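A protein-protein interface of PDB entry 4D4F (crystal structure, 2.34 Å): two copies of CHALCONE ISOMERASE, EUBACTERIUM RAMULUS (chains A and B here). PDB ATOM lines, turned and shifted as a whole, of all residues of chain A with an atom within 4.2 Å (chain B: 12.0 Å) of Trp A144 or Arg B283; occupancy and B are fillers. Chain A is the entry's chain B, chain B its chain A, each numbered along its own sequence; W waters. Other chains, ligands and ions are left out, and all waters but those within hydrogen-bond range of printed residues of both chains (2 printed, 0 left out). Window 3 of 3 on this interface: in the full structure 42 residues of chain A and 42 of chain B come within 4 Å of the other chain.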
ATOM      1  N   ARG A  10      15.304 -14.913  16.279  1.00  0.00           N
ATOM      2  CA  ARG A  10      15.577 -15.612  15.025  1.00  0.00           C
ATOM      3  C   ARG A  10      16.972 -15.233  14.613  1.00  0.00           C
ATOM      4  O   ARG A  10      17.277 -14.033  14.589  1.00  0.00           O
ATOM      5  CB  ARG A  10      14.607 -15.135  13.965  1.00  0.00           C
ATOM      6  CG  ARG A  10      14.777 -15.770  12.611  1.00  0.00           C
ATOM      7  CD  ARG A  10      13.887 -15.079  11.592  1.00  0.00           C
ATOM      8  NE  ARG A  10      13.873 -15.830  10.329  1.00  0.00           N
ATOM      9  CZ  ARG A  10      13.870 -15.280   9.109  1.00  0.00           C
ATOM     10  NH1 ARG A  10      13.856 -13.947   8.939  1.00  0.00           N
ATOM     11  NH2 ARG A  10      13.877 -16.077   8.059  1.00  0.00           N
ATOM     12  N   HIS A  75      15.444 -20.610  15.384  1.00  0.00           N
ATOM     13  CA  HIS A  75      14.635 -19.842  16.323  1.00  0.00           C
ATOM     14  C   HIS A  75      14.905 -20.282  17.762  1.00  0.00           C
ATOM     15  O   HIS A  75      14.641 -21.441  18.130  1.00  0.00           O
ATOM     16  CB  HIS A  75      13.153 -19.946  16.002  1.00  0.00           C
ATOM     17  CG  HIS A  75      12.748 -19.233  14.758  1.00  0.00           C
ATOM     18  ND1 HIS A  75      13.042 -19.711  13.500  1.00  0.00           N
ATOM     19  CD2 HIS A  75      12.004 -18.118  14.573  1.00  0.00           C
ATOM     20  CE1 HIS A  75      12.505 -18.912  12.591  1.00  0.00           C
ATOM     21  NE2 HIS A  75      11.879 -17.935  13.216  1.00  0.00           N
ATOM     22  N   PRO A 142      15.048 -10.001  16.360  1.00  0.00           N
ATOM     23  CA  PRO A 142      13.757 -10.428  16.922  1.00  0.00           C
ATOM     24  C   PRO A 142      13.080 -11.436  15.987  1.00  0.00           C
ATOM     25  O   PRO A 142      13.446 -11.547  14.829  1.00  0.00           O
ATOM     26  CB  PRO A 142      12.959  -9.122  17.036  1.00  0.00           C
ATOM     27  CG  PRO A 142      13.535  -8.238  16.004  1.00  0.00           C
ATOM     28  CD  PRO A 142      14.984  -8.631  15.819  1.00  0.00           C
ATOM     29  N   MET A 143      12.158 -12.213  16.520  1.00  0.00           N
ATOM     30  CA  MET A 143      11.465 -13.211  15.723  1.00  0.00           C
ATOM     31  C   MET A 143      10.539 -12.606  14.692  1.00  0.00           C
ATOM     32  O   MET A 143      10.092 -13.308  13.779  1.00  0.00           O
ATOM     33  CB  MET A 143      10.633 -14.125  16.605  1.00  0.00           C
ATOM     34  CG  MET A 143      11.452 -15.194  17.307  1.00  0.00           C
ATOM     35  SD  MET A 143      10.414 -16.501  17.985  1.00  0.00           S
ATOM     36  CE  MET A 143      11.730 -17.509  18.663  1.00  0.00           C
ATOM     37  N   TRP A 144      10.210 -11.330  14.875  1.00  0.00           N
ATOM     38  CA  TRP A 144       9.273 -10.643  13.985  1.00  0.00           C
ATOM     39  C   TRP A 144       9.910  -9.402  13.383  1.00  0.00           C
ATOM     40  O   TRP A 144      10.582  -8.630  14.060  1.00  0.00           O
ATOM     41  CB  TRP A 144       7.993 -10.266  14.720  1.00  0.00           C
ATOM     42  CG  TRP A 144       7.373 -11.421  15.341  1.00  0.00           C
ATOM     43  CD1 TRP A 144       6.435 -12.242  14.786  1.00  0.00           C
ATOM     44  CD2 TRP A 144       7.622 -11.926  16.645  1.00  0.00           C
ATOM     45  NE1 TRP A 144       6.072 -13.224  15.674  1.00  0.00           N
ATOM     46  CE2 TRP A 144       6.801 -13.074  16.813  1.00  0.00           C
ATOM     47  CE3 TRP A 144       8.471 -11.544  17.687  1.00  0.00           C
ATOM     48  CZ2 TRP A 144       6.800 -13.824  17.972  1.00  0.00           C
ATOM     49  CZ3 TRP A 144       8.460 -12.299  18.854  1.00  0.00           C
ATOM     50  CH2 TRP A 144       7.630 -13.422  18.980  1.00  0.00           C
ATOM     51  N   TRP A 145       9.661  -9.211  12.095  1.00  0.00           N
ATOM     52  CA  TRP A 145      10.238  -8.091  11.398  1.00  0.00           C
ATOM     53  C   TRP A 145       9.836  -6.791  12.060  1.00  0.00           C
ATOM     54  O   TRP A 145       8.691  -6.604  12.433  1.00  0.00           O
ATOM     55  CB  TRP A 145       9.812  -8.106   9.943  1.00  0.00           C
ATOM     56  CG  TRP A 145      10.402  -9.226   9.159  1.00  0.00           C
ATOM     57  CD1 TRP A 145       9.784 -10.395   8.765  1.00  0.00           C
ATOM     58  CD2 TRP A 145      11.715  -9.283   8.639  1.00  0.00           C
ATOM     59  NE1 TRP A 145      10.642 -11.163   8.017  1.00  0.00           N
ATOM     60  CE2 TRP A 145      11.835 -10.505   7.927  1.00  0.00           C
ATOM     61  CE3 TRP A 145      12.814  -8.424   8.703  1.00  0.00           C
ATOM     62  CZ2 TRP A 145      13.003 -10.883   7.311  1.00  0.00           C
ATOM     63  CZ3 TRP A 145      13.969  -8.786   8.053  1.00  0.00           C
ATOM     64  CH2 TRP A 145      14.060 -10.002   7.358  1.00  0.00           C
ATOM     65  N   GLU A 146      10.788  -5.889  12.205  1.00  0.00           N
ATOM     66  CA  GLU A 146      10.505  -4.615  12.836  1.00  0.00           C
ATOM     67  C   GLU A 146       9.848  -3.623  11.915  1.00  0.00           C
ATOM     68  O   GLU A 146       9.056  -2.823  12.365  1.00  0.00           O
ATOM     69  CB  GLU A 146      11.777  -4.016  13.450  1.00  0.00           C
ATOM     70  CG  GLU A 146      12.253  -4.857  14.627  1.00  0.00           C
ATOM     71  CD  GLU A 146      13.564  -4.424  15.251  1.00  0.00           C
ATOM     72  OE1 GLU A 146      14.397  -3.770  14.586  1.00  0.00           O
ATOM     73  OE2 GLU A 146      13.755  -4.793  16.436  1.00  0.00           O
ATOM     74  N   ARG A 163      13.250 -14.337  -2.899  1.00  0.00           N
ATOM     75  CA  ARG A 163      13.427 -13.639  -1.630  1.00  0.00           C
ATOM     76  C   ARG A 163      14.898 -13.326  -1.405  1.00  0.00           C
ATOM     77  O   ARG A 163      15.696 -14.222  -1.112  1.00  0.00           O
ATOM     78  CB  ARG A 163      12.854 -14.485  -0.484  1.00  0.00           C
ATOM     79  CG  ARG A 163      11.366 -14.684  -0.666  1.00  0.00           C
ATOM     80  CD  ARG A 163      10.717 -15.648   0.294  1.00  0.00           C
ATOM     81  NE  ARG A 163      10.734 -15.155   1.651  1.00  0.00           N
ATOM     82  CZ  ARG A 163       9.859 -15.467   2.615  1.00  0.00           C
ATOM     83  NH1 ARG A 163       8.783 -16.245   2.395  1.00  0.00           N
ATOM     84  NH2 ARG A 163      10.063 -14.955   3.829  1.00  0.00           N
ATOM     85  N   SER A 203      14.801  -5.460   9.939  1.00  0.00           N
ATOM     86  CA  SER A 203      14.971  -5.485  11.373  1.00  0.00           C
ATOM     87  C   SER A 203      16.399  -5.071  11.685  1.00  0.00           C
ATOM     88  O   SER A 203      17.320  -5.359  10.913  1.00  0.00           O
ATOM     89  CB  SER A 203      14.690  -6.884  11.966  1.00  0.00           C
ATOM     90  OG  SER A 203      13.294  -7.215  11.959  1.00  0.00           O
ATOM     91  N   TYR B 279       3.305 -27.051   2.420  1.00  0.00           N
ATOM     92  CA  TYR B 279       4.137 -25.994   1.900  1.00  0.00           C
ATOM     93  C   TYR B 279       4.228 -24.840   2.919  1.00  0.00           C
ATOM     94  O   TYR B 279       3.576 -23.776   2.784  1.00  0.00           O
ATOM     95  CB  TYR B 279       3.568 -25.536   0.550  1.00  0.00           C
ATOM     96  CG  TYR B 279       4.473 -24.666  -0.284  1.00  0.00           C
ATOM     97  CD1 TYR B 279       5.512 -25.217  -1.011  1.00  0.00           C
ATOM     98  CD2 TYR B 279       4.252 -23.289  -0.378  1.00  0.00           C
ATOM     99  CE1 TYR B 279       6.310 -24.430  -1.811  1.00  0.00           C
ATOM    100  CE2 TYR B 279       5.052 -22.495  -1.157  1.00  0.00           C
ATOM    101  CZ  TYR B 279       6.100 -23.062  -1.861  1.00  0.00           C
ATOM    102  OH  TYR B 279       6.917 -22.269  -2.635  1.00  0.00           O
ATOM    103  N   ILE B 280       5.040 -25.061   3.943  1.00  0.00           N
ATOM    104  CA  ILE B 280       5.259 -24.082   4.993  1.00  0.00           C
ATOM    105  C   ILE B 280       6.211 -23.015   4.471  1.00  0.00           C
ATOM    106  O   ILE B 280       7.252 -23.331   3.957  1.00  0.00           O
ATOM    107  CB  ILE B 280       5.890 -24.768   6.222  1.00  0.00           C
ATOM    108  CG1 ILE B 280       4.995 -25.927   6.694  1.00  0.00           C
ATOM    109  CG2 ILE B 280       6.178 -23.783   7.362  1.00  0.00           C
ATOM    110  CD1 ILE B 280       3.527 -25.564   6.773  1.00  0.00           C
ATOM    111  N   THR B 281       5.862 -21.752   4.615  1.00  0.00           N
ATOM    112  CA  THR B 281       6.637 -20.672   4.034  1.00  0.00           C
ATOM    113  C   THR B 281       7.559 -20.040   5.067  1.00  0.00           C
ATOM    114  O   THR B 281       7.208 -19.954   6.228  1.00  0.00           O
ATOM    115  CB  THR B 281       5.699 -19.580   3.450  1.00  0.00           C
ATOM    116  OG1 THR B 281       4.737 -19.163   4.426  1.00  0.00           O
ATOM    117  CG2 THR B 281       4.963 -20.138   2.259  1.00  0.00           C
ATOM    118  N   MET B 282       8.726 -19.582   4.610  1.00  0.00           N
ATOM    119  CA  MET B 282       9.686 -18.827   5.408  1.00  0.00           C
ATOM    120  C   MET B 282       9.040 -17.557   5.952  1.00  0.00           C
ATOM    121  O   MET B 282       8.262 -16.876   5.266  1.00  0.00           O
ATOM    122  CB  MET B 282      10.903 -18.441   4.553  1.00  0.00           C
ATOM    123  CG  MET B 282      12.073 -17.947   5.367  1.00  0.00           C
ATOM    124  SD  MET B 282      13.607 -17.629   4.497  1.00  0.00           S
ATOM    125  CE  MET B 282      13.066 -16.430   3.327  1.00  0.00           C
ATOM    126  N   ARG B 283       9.383 -17.247   7.190  1.00  0.00           N
ATOM    127  CA  ARG B 283       8.855 -16.103   7.911  1.00  0.00           C
ATOM    128  C   ARG B 283       9.663 -14.801   7.619  1.00  0.00           C
ATOM    129  O   ARG B 283      10.405 -14.739   6.620  1.00  0.00           O
ATOM    130  CB  ARG B 283       8.868 -16.424   9.424  1.00  0.00           C
ATOM    131  CG  ARG B 283       8.137 -17.703   9.839  1.00  0.00           C
ATOM    132  CD  ARG B 283       8.286 -18.035  11.342  1.00  0.00           C
ATOM    133  NE  ARG B 283       7.678 -16.956  12.119  1.00  0.00           N
ATOM    134  CZ  ARG B 283       8.327 -15.950  12.707  1.00  0.00           C
ATOM    135  NH1 ARG B 283       9.646 -15.884  12.743  1.00  0.00           N
ATOM    136  NH2 ARG B 283       7.630 -14.995  13.274  1.00  0.00           N
ATOM    137  OXT ARG B 283       9.618 -13.796   8.375  1.00  0.00           O
HETATM  138  O   HOH W   1      13.082 -14.185   6.137  1.00  0.00           O
HETATM  139  O   HOH W   2      10.827 -13.111  10.861  1.00  0.00           O
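Of the 9 printed residues of chain A, 6 touch a printed residue of chain B.
Printed residues of chain A that touch a printed residue of chain B: Arg A10, His A75, Met A143, Trp A144, Trp A145 and Arg A163.
Of the 5 printed residues of chain B, 2 touch a printed residue of chain A.
Printed residues of chain B that touch a printed residue of chain A: Met B282 and Arg B283.
Hydrophobic or aromatic side chains of chain B that line the printed part of chain A: Met B282.
The guanidinium group (NH1) of Arg A163 lies within hydrogen-bond range of the backbone carbonyl oxygen (O) of Met B282 (3.0 Å).
The chain-end carboxylate (O) of Arg B283 lies within salt-bridge range of the guanidinium group (NH2) of Arg A10, at 3.99 Å.
A ring nitrogen (NE2) of His A75 lies within hydrogen-bond range of the guanidinium group (NH1) of Arg B283.
The guanidinium group of Arg A163 is in salt-bridge range of the chain-end carboxylate of Arg B283 (2.8 Å).
NE1 of Trp A144 lies close to NH2 of Arg B283, 3.4 Å away.
O of Met A143 lies within hydrogen-bond range of NH1 of Arg B283 (2.8 Å).
OXT of Arg B283 is in hydrogen-bond range of NE1 of Trp A145, 2.8 Å away.
Printed residues of chain B within 4 Å of Arg A10: Met B282 and Arg B283.
No residue of chain B comes within 4 Å of Pro A142.
Of chain B, only Arg B283 (2.8 Å) comes within 4 Å of Met A143.
Trp A145 touches one residue of chain B.
Glu A146 touches none of the printed residues of chain B.
Printed residues of chain B within 4 Å of Arg A163: Met B282 (3.0 Å) and Arg B283 (2.8 Å).
Thr B281 touches none of the printed residues of chain A.
Printed residues of chain A within 4 Å of Met B282: Arg A10 and Arg A163.
The nearest printed residue of chain A that does not touch Arg B283 is Pro A142 (6.1 Å).
The nearest printed residue of chain B that does not touch His A75 is Met B282 (7.3 Å).
CG of Met B282 touches NH2 of Arg A10 (3.7 Å).
No position is printed for both chains.
Water W1 lies within hydrogen-bond range of the chain-end carboxylate of Arg B283 (2.8 Å) and the guanidinium group of Arg A10 (2.8 Å).
Water W2 lies within hydrogen-bond range of the chain-end carboxylate of Arg B283, the backbone carbonyl oxygen of Met A143 and the indole nitrogen of Trp A145.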
